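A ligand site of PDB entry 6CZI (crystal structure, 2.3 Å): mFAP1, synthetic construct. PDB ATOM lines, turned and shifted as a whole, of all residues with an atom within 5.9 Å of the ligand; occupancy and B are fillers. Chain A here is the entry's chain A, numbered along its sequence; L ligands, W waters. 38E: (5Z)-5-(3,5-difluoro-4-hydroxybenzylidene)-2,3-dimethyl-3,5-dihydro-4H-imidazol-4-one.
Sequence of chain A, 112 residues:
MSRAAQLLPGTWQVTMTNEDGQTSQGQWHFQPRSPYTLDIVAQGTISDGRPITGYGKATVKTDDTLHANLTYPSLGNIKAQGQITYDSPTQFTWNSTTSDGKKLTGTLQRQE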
ATOM      1  N   VAL A  14       5.519 -22.904 -18.237  1.00  0.00           N
ATOM      2  CA  VAL A  14       5.369 -21.679 -17.461  1.00  0.00           C
ATOM      3  C   VAL A  14       3.898 -21.309 -17.480  1.00  0.00           C
ATOM      4  O   VAL A  14       3.241 -21.369 -18.536  1.00  0.00           O
ATOM      5  CB  VAL A  14       6.240 -20.538 -18.016  1.00  0.00           C
ATOM      6  CG1 VAL A  14       6.058 -19.266 -17.166  1.00  0.00           C
ATOM      7  CG2 VAL A  14       7.727 -20.947 -18.019  1.00  0.00           C
ATOM      8  N   THR A  15       3.365 -21.019 -16.290  1.00  0.00           N
ATOM      9  CA  THR A  15       2.049 -20.433 -16.090  1.00  0.00           C
ATOM     10  C   THR A  15       2.214 -19.203 -15.232  1.00  0.00           C
ATOM     11  O   THR A  15       2.981 -19.211 -14.266  1.00  0.00           O
ATOM     12  CB  THR A  15       1.106 -21.404 -15.413  1.00  0.00           C
ATOM     13  OG1 THR A  15       1.090 -22.631 -16.132  1.00  0.00           O
ATOM     14  CG2 THR A  15      -0.283 -20.815 -15.386  1.00  0.00           C
ATOM     15  N   MET A  16       1.517 -18.134 -15.593  1.00  0.00           N
ATOM     16  CA  MET A  16       1.601 -16.898 -14.832  1.00  0.00           C
ATOM     17  C   MET A  16       0.209 -16.309 -14.674  1.00  0.00           C
ATOM     18  O   MET A  16      -0.723 -16.614 -15.438  1.00  0.00           O
ATOM     19  CB  MET A  16       2.550 -15.906 -15.507  1.00  0.00           C
ATOM     20  CG  MET A  16       4.034 -16.399 -15.707  1.00  0.00           C
ATOM     21  SD  MET A  16       5.030 -14.976 -16.140  1.00  0.00           S
ATOM     22  CE  MET A  16       6.638 -15.708 -16.602  1.00  0.00           C
ATOM     23  N   THR A  17       0.064 -15.465 -13.642  1.00  0.00           N
ATOM     24  CA  THR A  17      -1.034 -14.526 -13.509  1.00  0.00           C
ATOM     25  C   THR A  17      -0.455 -13.152 -13.262  1.00  0.00           C
ATOM     26  O   THR A  17       0.643 -13.019 -12.706  1.00  0.00           O
ATOM     27  CB  THR A  17      -2.030 -14.881 -12.364  1.00  0.00           C
ATOM     28  OG1 THR A  17      -1.341 -14.951 -11.113  1.00  0.00           O
ATOM     29  CG2 THR A  17      -2.770 -16.192 -12.645  1.00  0.00           C
ATOM     30  N   ASN A  18      -1.147 -12.135 -13.752  1.00  0.00           N
ATOM     31  CA  ASN A  18      -0.711 -10.747 -13.594  1.00  0.00           C
ATOM     32  C   ASN A  18      -1.753  -9.956 -12.792  1.00  0.00           C
ATOM     33  O   ASN A  18      -2.805 -10.475 -12.405  1.00  0.00           O
ATOM     34  CB  ASN A  18      -0.422 -10.095 -14.949  1.00  0.00           C
ATOM     35  CG  ASN A  18      -1.633  -9.966 -15.833  1.00  0.00           C
ATOM     36  OD1 ASN A  18      -2.784  -9.870 -15.352  1.00  0.00           O
ATOM     37  ND2 ASN A  18      -1.385  -9.906 -17.140  1.00  0.00           N
ATOM     38  N   GLN A  22      -5.285 -11.599 -15.577  1.00  0.00           N
ATOM     39  CA  GLN A  22      -5.053 -12.454 -16.726  1.00  0.00           C
ATOM     40  C   GLN A  22      -4.119 -13.600 -16.356  1.00  0.00           C
ATOM     41  O   GLN A  22      -3.332 -13.523 -15.413  1.00  0.00           O
ATOM     42  CB  GLN A  22      -4.452 -11.665 -17.880  1.00  0.00           C
ATOM     43  CG  GLN A  22      -5.266 -10.471 -18.305  1.00  0.00           C
ATOM     44  CD  GLN A  22      -4.502  -9.485 -19.170  1.00  0.00           C
ATOM     45  OE1 GLN A  22      -3.315  -9.265 -18.982  1.00  0.00           O
ATOM     46  NE2 GLN A  22      -5.194  -8.871 -20.100  1.00  0.00           N
ATOM     47  N   THR A  23      -4.180 -14.641 -17.160  1.00  0.00           N
ATOM     48  CA  THR A  23      -3.235 -15.733 -17.048  1.00  0.00           C
ATOM     49  C   THR A  23      -2.522 -15.933 -18.376  1.00  0.00           C
ATOM     50  O   THR A  23      -3.001 -15.519 -19.427  1.00  0.00           O
ATOM     51  CB  THR A  23      -3.925 -17.016 -16.636  1.00  0.00           C
ATOM     52  OG1 THR A  23      -4.878 -17.354 -17.638  1.00  0.00           O
ATOM     53  CG2 THR A  23      -4.582 -16.858 -15.292  1.00  0.00           C
ATOM     54  N   SER A  24      -1.380 -16.586 -18.295  1.00  0.00           N
ATOM     55  CA  SER A  24      -0.584 -16.900 -19.471  1.00  0.00           C
ATOM     56  C   SER A  24      -0.103 -18.334 -19.312  1.00  0.00           C
ATOM     57  O   SER A  24       0.060 -18.847 -18.211  1.00  0.00           O
ATOM     58  CB  SER A  24       0.591 -15.934 -19.651  1.00  0.00           C
ATOM     59  OG  SER A  24       1.475 -16.014 -18.553  1.00  0.00           O
ATOM     60  N   GLN A  25       0.082 -18.982 -20.445  1.00  0.00           N
ATOM     61  CA  GLN A  25       0.567 -20.353 -20.517  1.00  0.00           C
ATOM     62  C   GLN A  25       1.665 -20.397 -21.572  1.00  0.00           C
ATOM     63  O   GLN A  25       1.575 -19.688 -22.568  1.00  0.00           O
ATOM     64  CB  GLN A  25      -0.588 -21.298 -20.861  1.00  0.00           C
ATOM     65  CG  GLN A  25      -0.365 -22.743 -20.461  1.00  0.00           C
ATOM     66  N   GLY A  26       2.737 -21.162 -21.328  1.00  0.00           N
ATOM     67  CA  GLY A  26       3.833 -21.175 -22.284  1.00  0.00           C
ATOM     68  C   GLY A  26       5.038 -21.927 -21.775  1.00  0.00           C
ATOM     69  O   GLY A  26       4.925 -22.831 -20.941  1.00  0.00           O
ATOM     70  N   GLN A  27       6.196 -21.553 -22.298  1.00  0.00           N
ATOM     71  CA  GLN A  27       7.446 -22.221 -21.943  1.00  0.00           C
ATOM     72  C   GLN A  27       8.551 -21.207 -21.756  1.00  0.00           C
ATOM     73  O   GLN A  27       8.565 -20.138 -22.358  1.00  0.00           O
ATOM     74  CB  GLN A  27       7.928 -23.239 -23.019  1.00  0.00           C
ATOM     75  CG  GLN A  27       7.022 -24.414 -23.306  1.00  0.00           C
ATOM     76  CD  GLN A  27       5.815 -24.043 -24.154  1.00  0.00           C
ATOM     77  OE1 GLN A  27       5.867 -23.119 -25.007  1.00  0.00           O
ATOM     78  NE2 GLN A  27       4.708 -24.741 -23.911  1.00  0.00           N
ATOM     79  N   TRP A  28       9.534 -21.634 -20.969  1.00  0.00           N
ATOM     80  CA  TRP A  28      10.815 -20.970 -20.817  1.00  0.00           C
ATOM     81  C   TRP A  28      11.854 -22.033 -21.153  1.00  0.00           C
ATOM     82  O   TRP A  28      11.752 -23.183 -20.692  1.00  0.00           O
ATOM     83  CB  TRP A  28      11.049 -20.462 -19.370  1.00  0.00           C
ATOM     84  CG  TRP A  28      10.540 -19.062 -19.081  1.00  0.00           C
ATOM     85  CD1 TRP A  28       9.700 -18.335 -19.855  1.00  0.00           C
ATOM     86  CD2 TRP A  28      10.782 -18.282 -17.904  1.00  0.00           C
ATOM     87  NE1 TRP A  28       9.430 -17.130 -19.267  1.00  0.00           N
ATOM     88  CE2 TRP A  28      10.078 -17.075 -18.064  1.00  0.00           C
ATOM     89  CE3 TRP A  28      11.527 -18.495 -16.726  1.00  0.00           C
ATOM     90  CZ2 TRP A  28      10.098 -16.064 -17.099  1.00  0.00           C
ATOM     91  CZ3 TRP A  28      11.543 -17.477 -15.773  1.00  0.00           C
ATOM     92  CH2 TRP A  28      10.834 -16.279 -15.963  1.00  0.00           C
ATOM     93  N   ALA A  42      11.515 -17.219 -24.175  1.00  0.00           N
ATOM     94  CA  ALA A  42      10.169 -17.276 -23.625  1.00  0.00           C
ATOM     95  C   ALA A  42       9.140 -17.289 -24.746  1.00  0.00           C
ATOM     96  O   ALA A  42       9.254 -16.549 -25.735  1.00  0.00           O
ATOM     97  CB  ALA A  42       9.928 -16.090 -22.694  1.00  0.00           C
ATOM     98  N   GLN A  43       8.159 -18.162 -24.629  1.00  0.00           N
ATOM     99  CA  GLN A  43       7.141 -18.272 -25.659  1.00  0.00           C
ATOM    100  C   GLN A  43       5.833 -18.682 -24.985  1.00  0.00           C
ATOM    101  O   GLN A  43       5.837 -19.520 -24.081  1.00  0.00           O
ATOM    102  CB  GLN A  43       7.599 -19.301 -26.707  1.00  0.00           C
ATOM    103  CG  GLN A  43       6.821 -19.351 -27.992  1.00  0.00           C
ATOM    104  CD  GLN A  43       7.545 -20.179 -29.079  1.00  0.00           C
ATOM    105  OE1 GLN A  43       7.798 -19.676 -30.184  1.00  0.00           O
ATOM    106  NE2 GLN A  43       7.846 -21.455 -28.758  1.00  0.00           N
ATOM    107  N   GLY A  44       4.718 -18.067 -25.410  1.00  0.00           N
ATOM    108  CA  GLY A  44       3.428 -18.411 -24.823  1.00  0.00           C
ATOM    109  C   GLY A  44       2.320 -17.488 -25.305  1.00  0.00           C
ATOM    110  O   GLY A  44       2.476 -16.787 -26.305  1.00  0.00           O
ATOM    111  N   THR A  45       1.214 -17.477 -24.554  1.00  0.00           N
ATOM    112  CA  THR A  45       0.044 -16.684 -24.894  1.00  0.00           C
ATOM    113  C   THR A  45      -0.601 -16.161 -23.624  1.00  0.00           C
ATOM    114  O   THR A  45      -0.769 -16.902 -22.652  1.00  0.00           O
ATOM    115  CB  THR A  45      -1.005 -17.505 -25.683  1.00  0.00           C
ATOM    116  OG1 THR A  45      -0.360 -18.237 -26.718  1.00  0.00           O
ATOM    117  CG2 THR A  45      -2.070 -16.594 -26.326  1.00  0.00           C
ATOM    118  N   ILE A  46      -1.027 -14.953 -23.656  1.00  0.00           N
ATOM    119  CA  ILE A  46      -1.765 -14.400 -22.543  1.00  0.00           C
ATOM    120  C   ILE A  46      -3.253 -14.614 -22.813  1.00  0.00           C
ATOM    121  O   ILE A  46      -3.677 -14.690 -23.969  1.00  0.00           O
ATOM    122  CB  ILE A  46      -1.398 -12.919 -22.338  1.00  0.00           C
ATOM    123  CG1 ILE A  46       0.123 -12.789 -22.193  1.00  0.00           C
ATOM    124  CG2 ILE A  46      -2.084 -12.333 -21.110  1.00  0.00           C
ATOM    125  CD1 ILE A  46       0.578 -11.390 -21.931  1.00  0.00           C
ATOM    126  N   ARG A  50      -2.881 -12.053 -26.479  1.00  0.00           N
ATOM    127  CA  ARG A  50      -1.581 -11.517 -26.855  1.00  0.00           C
ATOM    128  C   ARG A  50      -0.559 -12.651 -26.891  1.00  0.00           C
ATOM    129  O   ARG A  50      -0.461 -13.437 -25.936  1.00  0.00           O
ATOM    130  CB  ARG A  50      -1.137 -10.406 -25.882  1.00  0.00           C
ATOM    131  CG  ARG A  50      -1.733  -9.048 -26.239  1.00  0.00           C
ATOM    132  CD  ARG A  50      -1.311  -7.924 -25.293  1.00  0.00           C
ATOM    133  NE  ARG A  50      -1.720  -8.243 -23.941  1.00  0.00           N
ATOM    134  CZ  ARG A  50      -1.019  -7.927 -22.865  1.00  0.00           C
ATOM    135  NH1 ARG A  50       0.112  -7.278 -22.990  1.00  0.00           N
ATOM    136  NH2 ARG A  50      -1.450  -8.290 -21.653  1.00  0.00           N
ATOM    137  N   ILE A  52       3.202 -14.196 -26.598  1.00  0.00           N
ATOM    138  CA  ILE A  52       4.407 -13.898 -25.830  1.00  0.00           C
ATOM    139  C   ILE A  52       5.626 -14.403 -26.588  1.00  0.00           C
ATOM    140  O   ILE A  52       5.714 -15.593 -26.903  1.00  0.00           O
ATOM    141  CB  ILE A  52       4.371 -14.524 -24.435  1.00  0.00           C
ATOM    142  CG1 ILE A  52       3.191 -13.969 -23.643  1.00  0.00           C
ATOM    143  CG2 ILE A  52       5.704 -14.251 -23.719  1.00  0.00           C
ATOM    144  CD1 ILE A  52       3.037 -14.605 -22.273  1.00  0.00           C
ATOM    145  N   LEU A  70      14.075 -10.257 -18.081  1.00  0.00           N
ATOM    146  CA  LEU A  70      13.524 -10.642 -19.375  1.00  0.00           C
ATOM    147  C   LEU A  70      13.070  -9.400 -20.131  1.00  0.00           C
ATOM    148  O   LEU A  70      12.793  -8.358 -19.528  1.00  0.00           O
ATOM    149  CB  LEU A  70      12.347 -11.624 -19.213  1.00  0.00           C
ATOM    150  CG  LEU A  70      12.815 -13.018 -18.799  1.00  0.00           C
ATOM    151  CD1 LEU A  70      12.725 -13.216 -17.293  1.00  0.00           C
ATOM    152  CD2 LEU A  70      12.097 -14.104 -19.556  1.00  0.00           C
ATOM    153  N   TYR A  72      10.454  -8.440 -23.659  1.00  0.00           N
ATOM    154  CA  TYR A  72       9.366  -9.035 -24.444  1.00  0.00           C
ATOM    155  C   TYR A  72       9.053  -8.172 -25.665  1.00  0.00           C
ATOM    156  O   TYR A  72       8.159  -7.312 -25.636  1.00  0.00           O
ATOM    157  CB  TYR A  72       8.130  -9.226 -23.564  1.00  0.00           C
ATOM    158  CG  TYR A  72       8.263 -10.273 -22.462  1.00  0.00           C
ATOM    159  CD1 TYR A  72       8.624  -9.909 -21.175  1.00  0.00           C
ATOM    160  CD2 TYR A  72       8.039 -11.640 -22.708  1.00  0.00           C
ATOM    161  CE1 TYR A  72       8.726 -10.840 -20.146  1.00  0.00           C
ATOM    162  CE2 TYR A  72       8.152 -12.596 -21.690  1.00  0.00           C
ATOM    163  CZ  TYR A  72       8.503 -12.178 -20.401  1.00  0.00           C
ATOM    164  OH  TYR A  72       8.633 -13.080 -19.373  1.00  0.00           O
ATOM    165  N   LEU A  75       5.405  -7.698 -26.556  1.00  0.00           N
ATOM    166  CA  LEU A  75       4.561  -6.976 -25.597  1.00  0.00           C
ATOM    167  C   LEU A  75       4.993  -5.520 -25.456  1.00  0.00           C
ATOM    168  O   LEU A  75       5.092  -4.973 -24.346  1.00  0.00           O
ATOM    169  CB  LEU A  75       4.542  -7.664 -24.229  1.00  0.00           C
ATOM    170  CG  LEU A  75       4.154  -9.150 -24.221  1.00  0.00           C
ATOM    171  CD1 LEU A  75       4.127  -9.712 -22.789  1.00  0.00           C
ATOM    172  CD2 LEU A  75       2.771  -9.319 -24.855  1.00  0.00           C
ATOM    173  N   ILE A  78       8.138  -4.365 -23.096  1.00  0.00           N
ATOM    174  CA  ILE A  78       8.215  -4.283 -21.632  1.00  0.00           C
ATOM    175  C   ILE A  78       9.154  -5.372 -21.116  1.00  0.00           C
ATOM    176  O   ILE A  78       9.418  -6.390 -21.777  1.00  0.00           O
ATOM    177  CB  ILE A  78       6.838  -4.360 -20.953  1.00  0.00           C
ATOM    178  CG1 ILE A  78       6.158  -5.685 -21.265  1.00  0.00           C
ATOM    179  CG2 ILE A  78       5.913  -3.210 -21.375  1.00  0.00           C
ATOM    180  CD1 ILE A  78       6.235  -6.651 -20.154  1.00  0.00           C
ATOM    181  N   THR A  98       7.071  -6.175 -13.594  1.00  0.00           N
ATOM    182  CA  THR A  98       7.307  -5.699 -14.953  1.00  0.00           C
ATOM    183  C   THR A  98       7.805  -4.255 -14.904  1.00  0.00           C
ATOM    184  O   THR A  98       7.739  -3.574 -13.869  1.00  0.00           O
ATOM    185  CB  THR A  98       6.038  -5.755 -15.800  1.00  0.00           C
ATOM    186  OG1 THR A  98       5.030  -4.914 -15.230  1.00  0.00           O
ATOM    187  CG2 THR A  98       5.505  -7.194 -15.878  1.00  0.00           C
ATOM    188  N   LEU A 104       3.910  -9.706 -11.301  1.00  0.00           N
ATOM    189  CA  LEU A 104       3.712 -10.832 -12.206  1.00  0.00           C
ATOM    190  C   LEU A 104       4.388 -12.034 -11.572  1.00  0.00           C
ATOM    191  O   LEU A 104       5.593 -11.999 -11.331  1.00  0.00           O
ATOM    192  CB  LEU A 104       4.295 -10.525 -13.591  1.00  0.00           C
ATOM    193  CG  LEU A 104       4.353 -11.636 -14.654  1.00  0.00           C
ATOM    194  CD1 LEU A 104       2.949 -12.043 -15.081  1.00  0.00           C
ATOM    195  CD2 LEU A 104       5.244 -11.231 -15.896  1.00  0.00           C
HETATM  196  F1  38E L   1       0.705 -12.255 -18.215  1.00  0.00           F
HETATM  197  C2  38E L   1       1.964 -11.929 -18.533  1.00  0.00           C
HETATM  198  C1  38E L   1       2.306 -10.589 -18.545  1.00  0.00           C
HETATM  199  O1  38E L   1       1.388  -9.647 -18.231  1.00  0.00           O
HETATM  200  C3  38E L   1       2.893 -12.896 -18.859  1.00  0.00           C
HETATM  201  C4  38E L   1       4.209 -12.523 -19.151  1.00  0.00           C
HETATM  202  C5  38E L   1       4.542 -11.178 -19.183  1.00  0.00           C
HETATM  203  C   38E L   1       3.594 -10.233 -18.864  1.00  0.00           C
HETATM  204  F   38E L   1       3.902  -8.927 -18.859  1.00  0.00           F
HETATM  205  C6  38E L   1       5.252 -13.455 -19.538  1.00  0.00           C
HETATM  206  C7  38E L   1       5.091 -14.816 -19.750  1.00  0.00           C
HETATM  207  C9  38E L   1       6.198 -15.657 -20.233  1.00  0.00           C
HETATM  208  O   38E L   1       7.338 -15.309 -20.479  1.00  0.00           O
HETATM  209  N1  38E L   1       5.693 -16.892 -20.324  1.00  0.00           N
HETATM  210  C10 38E L   1       6.431 -18.070 -20.756  1.00  0.00           C
HETATM  211  C8  38E L   1       4.388 -16.861 -19.917  1.00  0.00           C
HETATM  212  N   38E L   1       4.005 -15.655 -19.584  1.00  0.00           N
HETATM  213  C11 38E L   1       3.550 -18.119 -19.889  1.00  0.00           C
HETATM  214  O   HOH W   1       0.695  -7.787 -19.875  1.00  0.00           O
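The side-chain hydroxyl (OG) of Ser 24 is in hydrogen-bond range of a nitrogen (N) of the ligand, 2.8 Å away.
OH of Tyr 72 lies within hydrogen-bond range of O of the ligand (2.8 Å).
O1 of the ligand is in hydrogen-bond range of ND2 of Asn 18 (3.0 Å).
The indole nitrogen (NE1) of Trp 28 sits at hydrogen-bond distance from an oxygen (O) of the ligand (3.0 Å).
The backbone NH (N) of Ser 24 lies within hydrogen-bond range of the backbone carbonyl oxygen (O) of Met 16, at 2.9 Å.
The backbone carbonyl oxygen (O) of Ile 78 lies within hydrogen-bond range of the backbone NH (N) of Tyr 72 (3.0 Å).
The side-chain amide nitrogen of Asn 18 is in hydrogen-bond range of the side-chain amide oxygen of Gln 22 (2.7 Å).
N of Ile 52 is in hydrogen-bond range of O of Gly 44, 2.7 Å away.
The backbone NH (N) of Gln 27 sits at hydrogen-bond distance from the backbone carbonyl oxygen (O) of Gln 43 (2.7 Å).
O of Gln 25 lies within hydrogen-bond range of N of Thr 45 (3.0 Å).
N of Val 14 lies within hydrogen-bond range of O of Gly 26, 2.8 Å away.
SD of Met 16 sits close to N of the ligand (3.7 Å).
Merely in contact with the ligand: Ile 52, Leu 104, Gln 27, Gln 25, Gly 26, Ala 42, Ile 78, Val 14, Gln 43, Ile 46, Thr 98 and Leu 75.
Hydrophobic or aromatic side chains within 4 Å of the ligand: Val 14, Met 16, Trp 28, Ala 42, Ile 46, Ile 52, Tyr 72, Leu 75, Ile 78 and Leu 104.
Water W1 bridges O1 of the ligand (2.6 Å) and NH2 of Arg 50 (2.8 Å).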
